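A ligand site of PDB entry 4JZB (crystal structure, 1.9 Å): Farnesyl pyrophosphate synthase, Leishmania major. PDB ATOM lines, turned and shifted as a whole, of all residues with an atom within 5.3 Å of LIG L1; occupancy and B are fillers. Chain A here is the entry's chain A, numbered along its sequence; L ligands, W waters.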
ATOM      1  N   GLY A  46       1.267  23.324   4.103  1.00  0.00           N
ATOM      2  CA  GLY A  46       0.883  22.708   2.830  1.00  0.00           C
ATOM      3  C   GLY A  46      -0.574  22.839   2.461  1.00  0.00           C
ATOM      4  O   GLY A  46      -0.966  22.482   1.343  1.00  0.00           O
ATOM      5  N   GLY A  47      -1.393  23.335   3.383  1.00  0.00           N
ATOM      6  CA  GLY A  47      -2.791  23.667   3.097  1.00  0.00           C
ATOM      7  C   GLY A  47      -2.892  25.049   2.449  1.00  0.00           C
ATOM      8  O   GLY A  47      -1.884  25.650   2.091  1.00  0.00           O
ATOM      9  N   LYS A  48      -4.122  25.538   2.312  1.00  0.00           N
ATOM     10  CA  LYS A  48      -4.366  26.833   1.648  1.00  0.00           C
ATOM     11  C   LYS A  48      -4.239  28.007   2.629  1.00  0.00           C
ATOM     12  O   LYS A  48      -4.132  29.171   2.212  1.00  0.00           O
ATOM     13  CB  LYS A  48      -5.760  26.851   1.004  1.00  0.00           C
ATOM     14  CG  LYS A  48      -6.023  25.685   0.025  1.00  0.00           C
ATOM     15  CD  LYS A  48      -7.466  25.730  -0.506  1.00  0.00           C
ATOM     16  CE  LYS A  48      -8.479  25.040   0.434  1.00  0.00           C
ATOM     17  NZ  LYS A  48      -8.301  23.554   0.455  1.00  0.00           N
ATOM     18  N   TYR A  49      -4.292  27.700   3.924  1.00  0.00           N
ATOM     19  CA  TYR A  49      -4.272  28.699   5.007  1.00  0.00           C
ATOM     20  C   TYR A  49      -5.450  29.678   5.003  1.00  0.00           C
ATOM     21  O   TYR A  49      -5.346  30.785   5.551  1.00  0.00           O
ATOM     22  CB  TYR A  49      -2.931  29.466   5.061  1.00  0.00           C
ATOM     23  CG  TYR A  49      -1.703  28.594   4.932  1.00  0.00           C
ATOM     24  CD1 TYR A  49      -0.986  28.528   3.735  1.00  0.00           C
ATOM     25  CD2 TYR A  49      -1.266  27.810   6.005  1.00  0.00           C
ATOM     26  CE1 TYR A  49       0.153  27.719   3.616  1.00  0.00           C
ATOM     27  CE2 TYR A  49      -0.142  26.994   5.897  1.00  0.00           C
ATOM     28  CZ  TYR A  49       0.566  26.958   4.707  1.00  0.00           C
ATOM     29  OH  TYR A  49       1.683  26.145   4.592  1.00  0.00           O
ATOM     30  N   ARG A  51      -8.187  29.623   6.797  1.00  0.00           N
ATOM     31  CA  ARG A  51      -8.597  29.953   8.183  1.00  0.00           C
ATOM     32  C   ARG A  51      -7.652  30.957   8.845  1.00  0.00           C
ATOM     33  O   ARG A  51      -8.086  32.005   9.330  1.00  0.00           O
ATOM     34  CB  ARG A  51      -8.716  28.690   9.042  1.00  0.00           C
ATOM     35  CG  ARG A  51      -9.794  27.727   8.606  1.00  0.00           C
ATOM     36  CD  ARG A  51      -9.596  26.353   9.281  1.00  0.00           C
ATOM     37  NE  ARG A  51     -10.448  25.322   8.692  1.00  0.00           N
ATOM     38  CZ  ARG A  51     -10.175  24.655   7.570  1.00  0.00           C
ATOM     39  NH1 ARG A  51      -9.057  24.904   6.882  1.00  0.00           N
ATOM     40  NH2 ARG A  51     -11.026  23.732   7.124  1.00  0.00           N
ATOM     41  N   GLU A  88      -4.978  27.077  12.446  1.00  0.00           N
ATOM     42  CA  GLU A  88      -4.234  26.161  11.583  1.00  0.00           C
ATOM     43  C   GLU A  88      -3.789  24.905  12.345  1.00  0.00           C
ATOM     44  O   GLU A  88      -3.831  23.807  11.814  1.00  0.00           O
ATOM     45  CB  GLU A  88      -3.049  26.849  10.909  1.00  0.00           C
ATOM     46  CG  GLU A  88      -3.445  27.907   9.835  1.00  0.00           C
ATOM     47  CD  GLU A  88      -4.278  27.322   8.695  1.00  0.00           C
ATOM     48  OE1 GLU A  88      -4.054  26.154   8.316  1.00  0.00           O
ATOM     49  OE2 GLU A  88      -5.168  28.033   8.187  1.00  0.00           O
ATOM     50  N   GLN A  91      -6.923  22.796  12.999  1.00  0.00           N
ATOM     51  CA  GLN A  91      -7.075  22.105  11.722  1.00  0.00           C
ATOM     52  C   GLN A  91      -6.091  20.925  11.640  1.00  0.00           C
ATOM     53  O   GLN A  91      -6.506  19.796  11.360  1.00  0.00           O
ATOM     54  CB  GLN A  91      -6.881  23.102  10.558  1.00  0.00           C
ATOM     55  CG  GLN A  91      -6.675  22.493   9.150  1.00  0.00           C
ATOM     56  CD  GLN A  91      -7.945  21.925   8.511  1.00  0.00           C
ATOM     57  OE1 GLN A  91      -8.080  21.918   7.265  1.00  0.00           O
ATOM     58  NE2 GLN A  91      -8.864  21.439   9.332  1.00  0.00           N
ATOM     59  N   LEU A  95      -7.190  16.990  11.256  1.00  0.00           N
ATOM     60  CA  LEU A  95      -6.839  16.211  10.059  1.00  0.00           C
ATOM     61  C   LEU A  95      -6.001  14.982  10.379  1.00  0.00           C
ATOM     62  O   LEU A  95      -6.202  13.928   9.772  1.00  0.00           O
ATOM     63  CB  LEU A  95      -6.178  17.075   8.990  1.00  0.00           C
ATOM     64  CG  LEU A  95      -6.931  18.305   8.462  1.00  0.00           C
ATOM     65  CD1 LEU A  95      -6.223  18.873   7.230  1.00  0.00           C
ATOM     66  CD2 LEU A  95      -8.410  18.037   8.167  1.00  0.00           C
ATOM     67  N   ARG A 107      -2.714  13.236   2.183  1.00  0.00           N
ATOM     68  CA  ARG A 107      -3.176  14.539   2.668  1.00  0.00           C
ATOM     69  C   ARG A 107      -2.235  15.617   2.151  1.00  0.00           C
ATOM     70  O   ARG A 107      -1.023  15.509   2.330  1.00  0.00           O
ATOM     71  CB  ARG A 107      -3.187  14.561   4.213  1.00  0.00           C
ATOM     72  CG  ARG A 107      -3.426  15.958   4.827  1.00  0.00           C
ATOM     73  CD  ARG A 107      -4.871  16.436   4.644  1.00  0.00           C
ATOM     74  NE  ARG A 107      -5.844  15.644   5.392  1.00  0.00           N
ATOM     75  CZ  ARG A 107      -7.165  15.783   5.284  1.00  0.00           C
ATOM     76  NH1 ARG A 107      -7.663  16.684   4.457  1.00  0.00           N
ATOM     77  NH2 ARG A 107      -7.980  15.024   5.997  1.00  0.00           N
ATOM     78  N   ARG A 108      -2.797  16.666   1.529  1.00  0.00           N
ATOM     79  CA  ARG A 108      -2.033  17.787   0.980  1.00  0.00           C
ATOM     80  C   ARG A 108      -0.894  17.315   0.054  1.00  0.00           C
ATOM     81  O   ARG A 108       0.198  17.881   0.075  1.00  0.00           O
ATOM     82  CB  ARG A 108      -1.485  18.703   2.092  1.00  0.00           C
ATOM     83  CG  ARG A 108      -2.559  19.500   2.831  1.00  0.00           C
ATOM     84  CD  ARG A 108      -2.049  19.985   4.190  1.00  0.00           C
ATOM     85  NE  ARG A 108      -3.070  20.725   4.942  1.00  0.00           N
ATOM     86  CZ  ARG A 108      -2.944  21.100   6.216  1.00  0.00           C
ATOM     87  NH1 ARG A 108      -1.830  20.814   6.886  1.00  0.00           N
ATOM     88  NH2 ARG A 108      -3.919  21.769   6.826  1.00  0.00           N
ATOM     89  N   THR A 208     -17.766  21.474  10.318  1.00  0.00           N
ATOM     90  CA  THR A 208     -16.984  22.355   9.442  1.00  0.00           C
ATOM     91  C   THR A 208     -17.211  23.851   9.614  1.00  0.00           C
ATOM     92  O   THR A 208     -16.255  24.619   9.743  1.00  0.00           O
ATOM     93  CB  THR A 208     -17.165  21.958   7.954  1.00  0.00           C
ATOM     94  OG1 THR A 208     -16.619  20.646   7.772  1.00  0.00           O
ATOM     95  CG2 THR A 208     -16.479  22.954   6.986  1.00  0.00           C
ATOM     96  N   TYR A 211     -15.525  25.931  12.883  1.00  0.00           N
ATOM     97  CA  TYR A 211     -14.081  26.115  12.934  1.00  0.00           C
ATOM     98  C   TYR A 211     -13.477  26.718  11.656  1.00  0.00           C
ATOM     99  O   TYR A 211     -12.397  27.310  11.713  1.00  0.00           O
ATOM    100  CB  TYR A 211     -13.366  24.834  13.377  1.00  0.00           C
ATOM    101  CG  TYR A 211     -12.898  23.883  12.301  1.00  0.00           C
ATOM    102  CD1 TYR A 211     -11.564  23.913  11.851  1.00  0.00           C
ATOM    103  CD2 TYR A 211     -13.750  22.921  11.754  1.00  0.00           C
ATOM    104  CE1 TYR A 211     -11.110  23.020  10.882  1.00  0.00           C
ATOM    105  CE2 TYR A 211     -13.295  22.019  10.781  1.00  0.00           C
ATOM    106  CZ  TYR A 211     -11.979  22.083  10.348  1.00  0.00           C
ATOM    107  OH  TYR A 211     -11.526  21.199   9.383  1.00  0.00           O
ATOM    108  N   THR A 212     -14.173  26.600  10.534  1.00  0.00           N
ATOM    109  CA  THR A 212     -13.631  27.058   9.241  1.00  0.00           C
ATOM    110  C   THR A 212     -14.077  28.485   8.877  1.00  0.00           C
ATOM    111  O   THR A 212     -13.328  29.218   8.201  1.00  0.00           O
ATOM    112  CB  THR A 212     -13.928  26.039   8.096  1.00  0.00           C
ATOM    113  OG1 THR A 212     -13.507  24.733   8.504  1.00  0.00           O
ATOM    114  CG2 THR A 212     -13.180  26.397   6.799  1.00  0.00           C
ATOM    115  N   PHE A 246     -19.088  25.409   1.781  1.00  0.00           N
ATOM    116  CA  PHE A 246     -17.698  24.970   1.718  1.00  0.00           C
ATOM    117  C   PHE A 246     -17.575  23.454   1.877  1.00  0.00           C
ATOM    118  O   PHE A 246     -16.811  22.805   1.159  1.00  0.00           O
ATOM    119  CB  PHE A 246     -16.856  25.718   2.758  1.00  0.00           C
ATOM    120  CG  PHE A 246     -15.423  25.254   2.844  1.00  0.00           C
ATOM    121  CD1 PHE A 246     -15.054  24.241   3.732  1.00  0.00           C
ATOM    122  CD2 PHE A 246     -14.437  25.860   2.066  1.00  0.00           C
ATOM    123  CE1 PHE A 246     -13.730  23.819   3.823  1.00  0.00           C
ATOM    124  CE2 PHE A 246     -13.099  25.454   2.151  1.00  0.00           C
ATOM    125  CZ  PHE A 246     -12.744  24.425   3.045  1.00  0.00           C
ATOM    126  N   GLN A 247     -18.318  22.878   2.825  1.00  0.00           N
ATOM    127  CA  GLN A 247     -18.313  21.424   2.992  1.00  0.00           C
ATOM    128  C   GLN A 247     -19.039  20.673   1.871  1.00  0.00           C
ATOM    129  O   GLN A 247     -18.641  19.566   1.496  1.00  0.00           O
ATOM    130  CB  GLN A 247     -18.870  21.003   4.342  1.00  0.00           C
ATOM    131  CG  GLN A 247     -18.677  19.518   4.634  1.00  0.00           C
ATOM    132  CD  GLN A 247     -17.204  19.100   4.659  1.00  0.00           C
ATOM    133  OE1 GLN A 247     -16.375  19.788   5.231  1.00  0.00           O
ATOM    134  NE2 GLN A 247     -16.894  17.976   4.030  1.00  0.00           N
ATOM    135  N   ASP A 250     -16.503  20.412  -0.704  1.00  0.00           N
ATOM    136  CA  ASP A 250     -15.620  19.308  -0.333  1.00  0.00           C
ATOM    137  C   ASP A 250     -16.234  17.947  -0.706  1.00  0.00           C
ATOM    138  O   ASP A 250     -15.538  17.091  -1.272  1.00  0.00           O
ATOM    139  CB  ASP A 250     -15.271  19.361   1.160  1.00  0.00           C
ATOM    140  CG  ASP A 250     -14.167  18.397   1.524  1.00  0.00           C
ATOM    141  OD1 ASP A 250     -13.012  18.627   1.107  1.00  0.00           O
ATOM    142  OD2 ASP A 250     -14.457  17.403   2.236  1.00  0.00           O
ATOM    143  N   LYS A 264      -5.691  14.799  -1.881  1.00  0.00           N
ATOM    144  CA  LYS A 264      -6.178  13.767  -0.956  1.00  0.00           C
ATOM    145  C   LYS A 264      -7.058  12.784  -1.714  1.00  0.00           C
ATOM    146  O   LYS A 264      -7.634  13.148  -2.741  1.00  0.00           O
ATOM    147  CB  LYS A 264      -6.953  14.399   0.221  1.00  0.00           C
ATOM    148  CG  LYS A 264      -8.249  15.141  -0.166  1.00  0.00           C
ATOM    149  CD  LYS A 264      -8.749  16.024   0.970  1.00  0.00           C
ATOM    150  CE  LYS A 264     -10.085  16.670   0.609  1.00  0.00           C
ATOM    151  NZ  LYS A 264     -10.463  17.777   1.550  1.00  0.00           N
ATOM    152  N   ARG A 360     -14.163  27.703  -5.723  1.00  0.00           N
ATOM    153  CA  ARG A 360     -12.817  27.167  -5.513  1.00  0.00           C
ATOM    154  C   ARG A 360     -12.678  25.814  -6.215  1.00  0.00           C
ATOM    155  O   ARG A 360     -13.666  25.098  -6.407  1.00  0.00           O
ATOM    156  CB  ARG A 360     -12.465  27.042  -4.023  1.00  0.00           C
ATOM    157  CG  ARG A 360     -13.229  25.954  -3.291  1.00  0.00           C
ATOM    158  CD  ARG A 360     -13.055  26.045  -1.776  1.00  0.00           C
ATOM    159  NE  ARG A 360     -13.831  25.014  -1.095  1.00  0.00           N
ATOM    160  CZ  ARG A 360     -13.342  23.850  -0.664  1.00  0.00           C
ATOM    161  NH1 ARG A 360     -12.053  23.542  -0.852  1.00  0.00           N
ATOM    162  NH2 ARG A 360     -14.135  22.992  -0.039  1.00  0.00           N
ATOM    163  N   LYS A 362     -10.044  23.559  -5.304  1.00  0.00           N
ATOM    164  CA  LYS A 362      -9.423  22.637  -4.343  1.00  0.00           C
ATOM    165  C   LYS A 362      -9.472  23.198  -2.916  1.00  0.00           C
ATOM    166  O   LYS A 362      -9.021  22.539  -1.977  1.00  0.00           O
ATOM    167  CB  LYS A 362      -7.970  22.312  -4.733  1.00  0.00           C
ATOM    168  CG  LYS A 362      -7.007  23.508  -4.696  1.00  0.00           C
ATOM    169  CD  LYS A 362      -5.546  23.061  -4.615  1.00  0.00           C
ATOM    170  CE  LYS A 362      -5.147  22.698  -3.179  1.00  0.00           C
ATOM    171  NZ  LYS A 362      -3.690  22.385  -3.054  1.00  0.00           N
ATOM    172  OXT LYS A 362      -9.941  24.313  -2.686  1.00  0.00           O
HETATM  173  C1  LIG L   1     -10.272  20.274   4.744  1.00  0.00           C
HETATM  174  O1  LIG L   1     -10.074  21.683   4.912  1.00  0.00           O
HETATM  175  C2  LIG L   1     -11.361  19.785   5.693  1.00  0.00           C
HETATM  176  C3  LIG L   1     -12.691  20.470   5.457  1.00  0.00           C
HETATM  177  C4  LIG L   1     -13.335  20.353   4.299  1.00  0.00           C
HETATM  178  C5  LIG L   1     -13.303  21.272   6.551  1.00  0.00           C
HETATM  179  P1  LIG L   1      -9.262  22.538   3.826  1.00  0.00           P
HETATM  180  O2  LIG L   1      -9.335  23.986   4.263  1.00  0.00           O
HETATM  181  O3  LIG L   1      -9.761  22.181   2.437  1.00  0.00           O
HETATM  182  O4  LIG L   1      -7.770  21.928   3.969  1.00  0.00           O
HETATM  183  P2  LIG L   1      -6.344  22.701   3.961  1.00  0.00           P
HETATM  184  O5  LIG L   1      -6.449  23.899   3.028  1.00  0.00           O
HETATM  185  O6  LIG L   1      -6.172  23.068   5.417  1.00  0.00           O
HETATM  186  O7  LIG L   1      -5.429  21.608   3.465  1.00  0.00           O
HETATM  187  C1  LG2 L   2     -11.996  16.349   6.831  1.00  0.00           C
HETATM  188  C2  LG2 L   2     -12.711  16.015   5.510  1.00  0.00           C
HETATM  189  P1  LG2 L   2     -14.017  14.757   5.726  1.00  0.00           P
HETATM  190  O1  LG2 L   2     -13.401  13.455   6.167  1.00  0.00           O
HETATM  191  O2  LG2 L   2     -14.684  14.658   4.369  1.00  0.00           O
HETATM  192  N1  LG2 L   2     -12.768  16.925   7.941  1.00  0.00           N
HETATM  193  O3  LG2 L   2     -14.970  15.300   6.749  1.00  0.00           O
HETATM  194  C3  LG2 L   2     -13.685  17.911   7.754  1.00  0.00           C
HETATM  195  O4  LG2 L   2     -13.354  17.202   4.977  1.00  0.00           O
HETATM  196  C4  LG2 L   2     -14.387  18.446   8.824  1.00  0.00           C
HETATM  197  P2  LG2 L   2     -11.370  15.545   4.354  1.00  0.00           P
HETATM  198  C5  LG2 L   2     -14.145  17.969  10.118  1.00  0.00           C
HETATM  199  O5  LG2 L   2     -12.029  15.238   3.034  1.00  0.00           O
HETATM  200  C6  LG2 L   2     -13.198  16.952  10.308  1.00  0.00           C
HETATM  201  O6  LG2 L   2     -10.693  14.348   4.980  1.00  0.00           O
HETATM  202  C7  LG2 L   2     -12.522  16.465   9.181  1.00  0.00           C
HETATM  203  O7  LG2 L   2     -10.447  16.753   4.290  1.00  0.00           O
HETATM  204  C8  LG2 L   2     -12.903  16.413  11.670  1.00  0.00           C
HETATM  205  C9  LG2 L   2     -13.126  17.191  12.805  1.00  0.00           C
HETATM  206  C10 LG2 L   2     -12.859  16.683  14.077  1.00  0.00           C
HETATM  207  C11 LG2 L   2     -12.350  15.388  14.236  1.00  0.00           C
HETATM  208  C12 LG2 L   2     -12.118  14.604  13.091  1.00  0.00           C
HETATM  209  C13 LG2 L   2     -12.415  15.113  11.833  1.00  0.00           C
HETATM  210  O   HOH W   1      -4.337  25.254   5.793  1.00  0.00           O
HETATM  211  O   HOH W   2      -5.380  21.936   0.669  1.00  0.00           O
HETATM  212  O   HOH W   3     -11.899  21.183   0.838  1.00  0.00           O
HETATM  213  O   HOH W   4      -8.684  19.890   1.408  1.00  0.00           O
HETATM  214  O   HOH W   5      -7.387  26.341   4.145  1.00  0.00           O
HETATM  215  O   HOH W   6     -10.170  26.328   3.873  1.00  0.00           O
HETATM  216  O   HOH W   7      -6.520  19.199   3.087  1.00  0.00           O
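Water W7 lies within hydrogen-bond range of an oxygen (O7) of LIG L1 (2.7 Å) and the guanidinium group (NH1) of Arg 107 (3.1 Å).
Water W4 bridges an oxygen (O3) of LIG L1 (2.7 Å) and the side-chain amino group of Lys 264 (2.8 Å).
Water W2 bridges O7 of LIG L1 (2.8 Å) and NZ of Lys 48 (3.3 Å).
Water W5 lies within hydrogen-bond range of O5 of LIG L1 (2.8 Å) and N of Tyr 49 (3.4 Å).
Water W3 lies within hydrogen-bond range of the side-chain carboxylate of Asp 250, an oxygen (O3) of LIG L1 and the guanidinium group of Arg 360.
Water W1 lies within hydrogen-bond range of the side-chain carboxylate of Glu 88 (2.7 Å), an oxygen (O6) of LIG L1 (2.9 Å), the backbone NH of Tyr 49 (3.1 Å) and the backbone NH of Lys 48 (3.5 Å).
Gly 47 touches LIG L1.
Thr 208 touches LIG L1 (OG1 to C5, 3.6 Å).
OH of Tyr 211 touches C5 of LIG L1, 3.3 Å away.
OG1 of Thr 212 touches C5 of LIG L1 (3.98 Å).
CE1 of Phe 246 touches C4 of LIG L1, 3.5 Å away.
Gln 247 touches LIG L1.
Asp 250 touches LIG L1.
Hydrophobic or aromatic side chains within 4 Å of LIG L1: Phe 246.
Within 4 Å of LIG L1: Gly 47, Lys 48, Arg 51, Gln 91, Arg 108, Thr 208, Tyr 211, Thr 212, Phe 246, Gln 247 and Asp 250.
NH1 of Arg 51 is in hydrogen-bond range of OE1 of Gln 91.
The guanidinium group (NH2) of Arg 51 lies within hydrogen-bond range of the side-chain hydroxyl (OG1) of Thr 212 (3.0 Å).
NZ of Lys 48 lies within salt-bridge range of O of Lys 362, at 2.7 Å.
NE2 of Gln 91 sits at hydrogen-bond distance from OH of Tyr 211, at 2.7 Å.
OD2 of Asp 250 sits close to NE2 of Gln 247.
The side-chain amide oxygen (OE1) of Gln 247 is in hydrogen-bond range of the side-chain hydroxyl (OG1) of Thr 208, at 2.7 Å.
The side-chain carboxylate (OD1) of Asp 250 lies within salt-bridge range of the side-chain amino group (NZ) of Lys 264 (2.7 Å).
The backbone carbonyl oxygen (O) of Thr 208 lies within hydrogen-bond range of the side-chain hydroxyl (OG1) of Thr 212.
The guanidinium group of Arg 51 is in salt-bridge range of an oxygen (O2) of LIG L1, at 2.8 Å.
N of Lys 48 lies within hydrogen-bond range of O5 of LIG L1 (2.9 Å).
The side-chain amino group (NZ) of Lys 48 is in salt-bridge range of an oxygen (O3) of LIG L1, at 2.8 Å.
OE1 of Gln 91 sits close to O6 of LIG L1 (2.9 Å).
An oxygen (O7) of LIG L1 is in salt-bridge range of the guanidinium group (NE) of Arg 108 (2.9 Å).
O7 of LG2 L2 is in salt-bridge range of NZ of Lys 264 (2.9 Å).
O7 of LG2 L2 is in salt-bridge range of NH1 of Arg 107 (2.8 Å).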
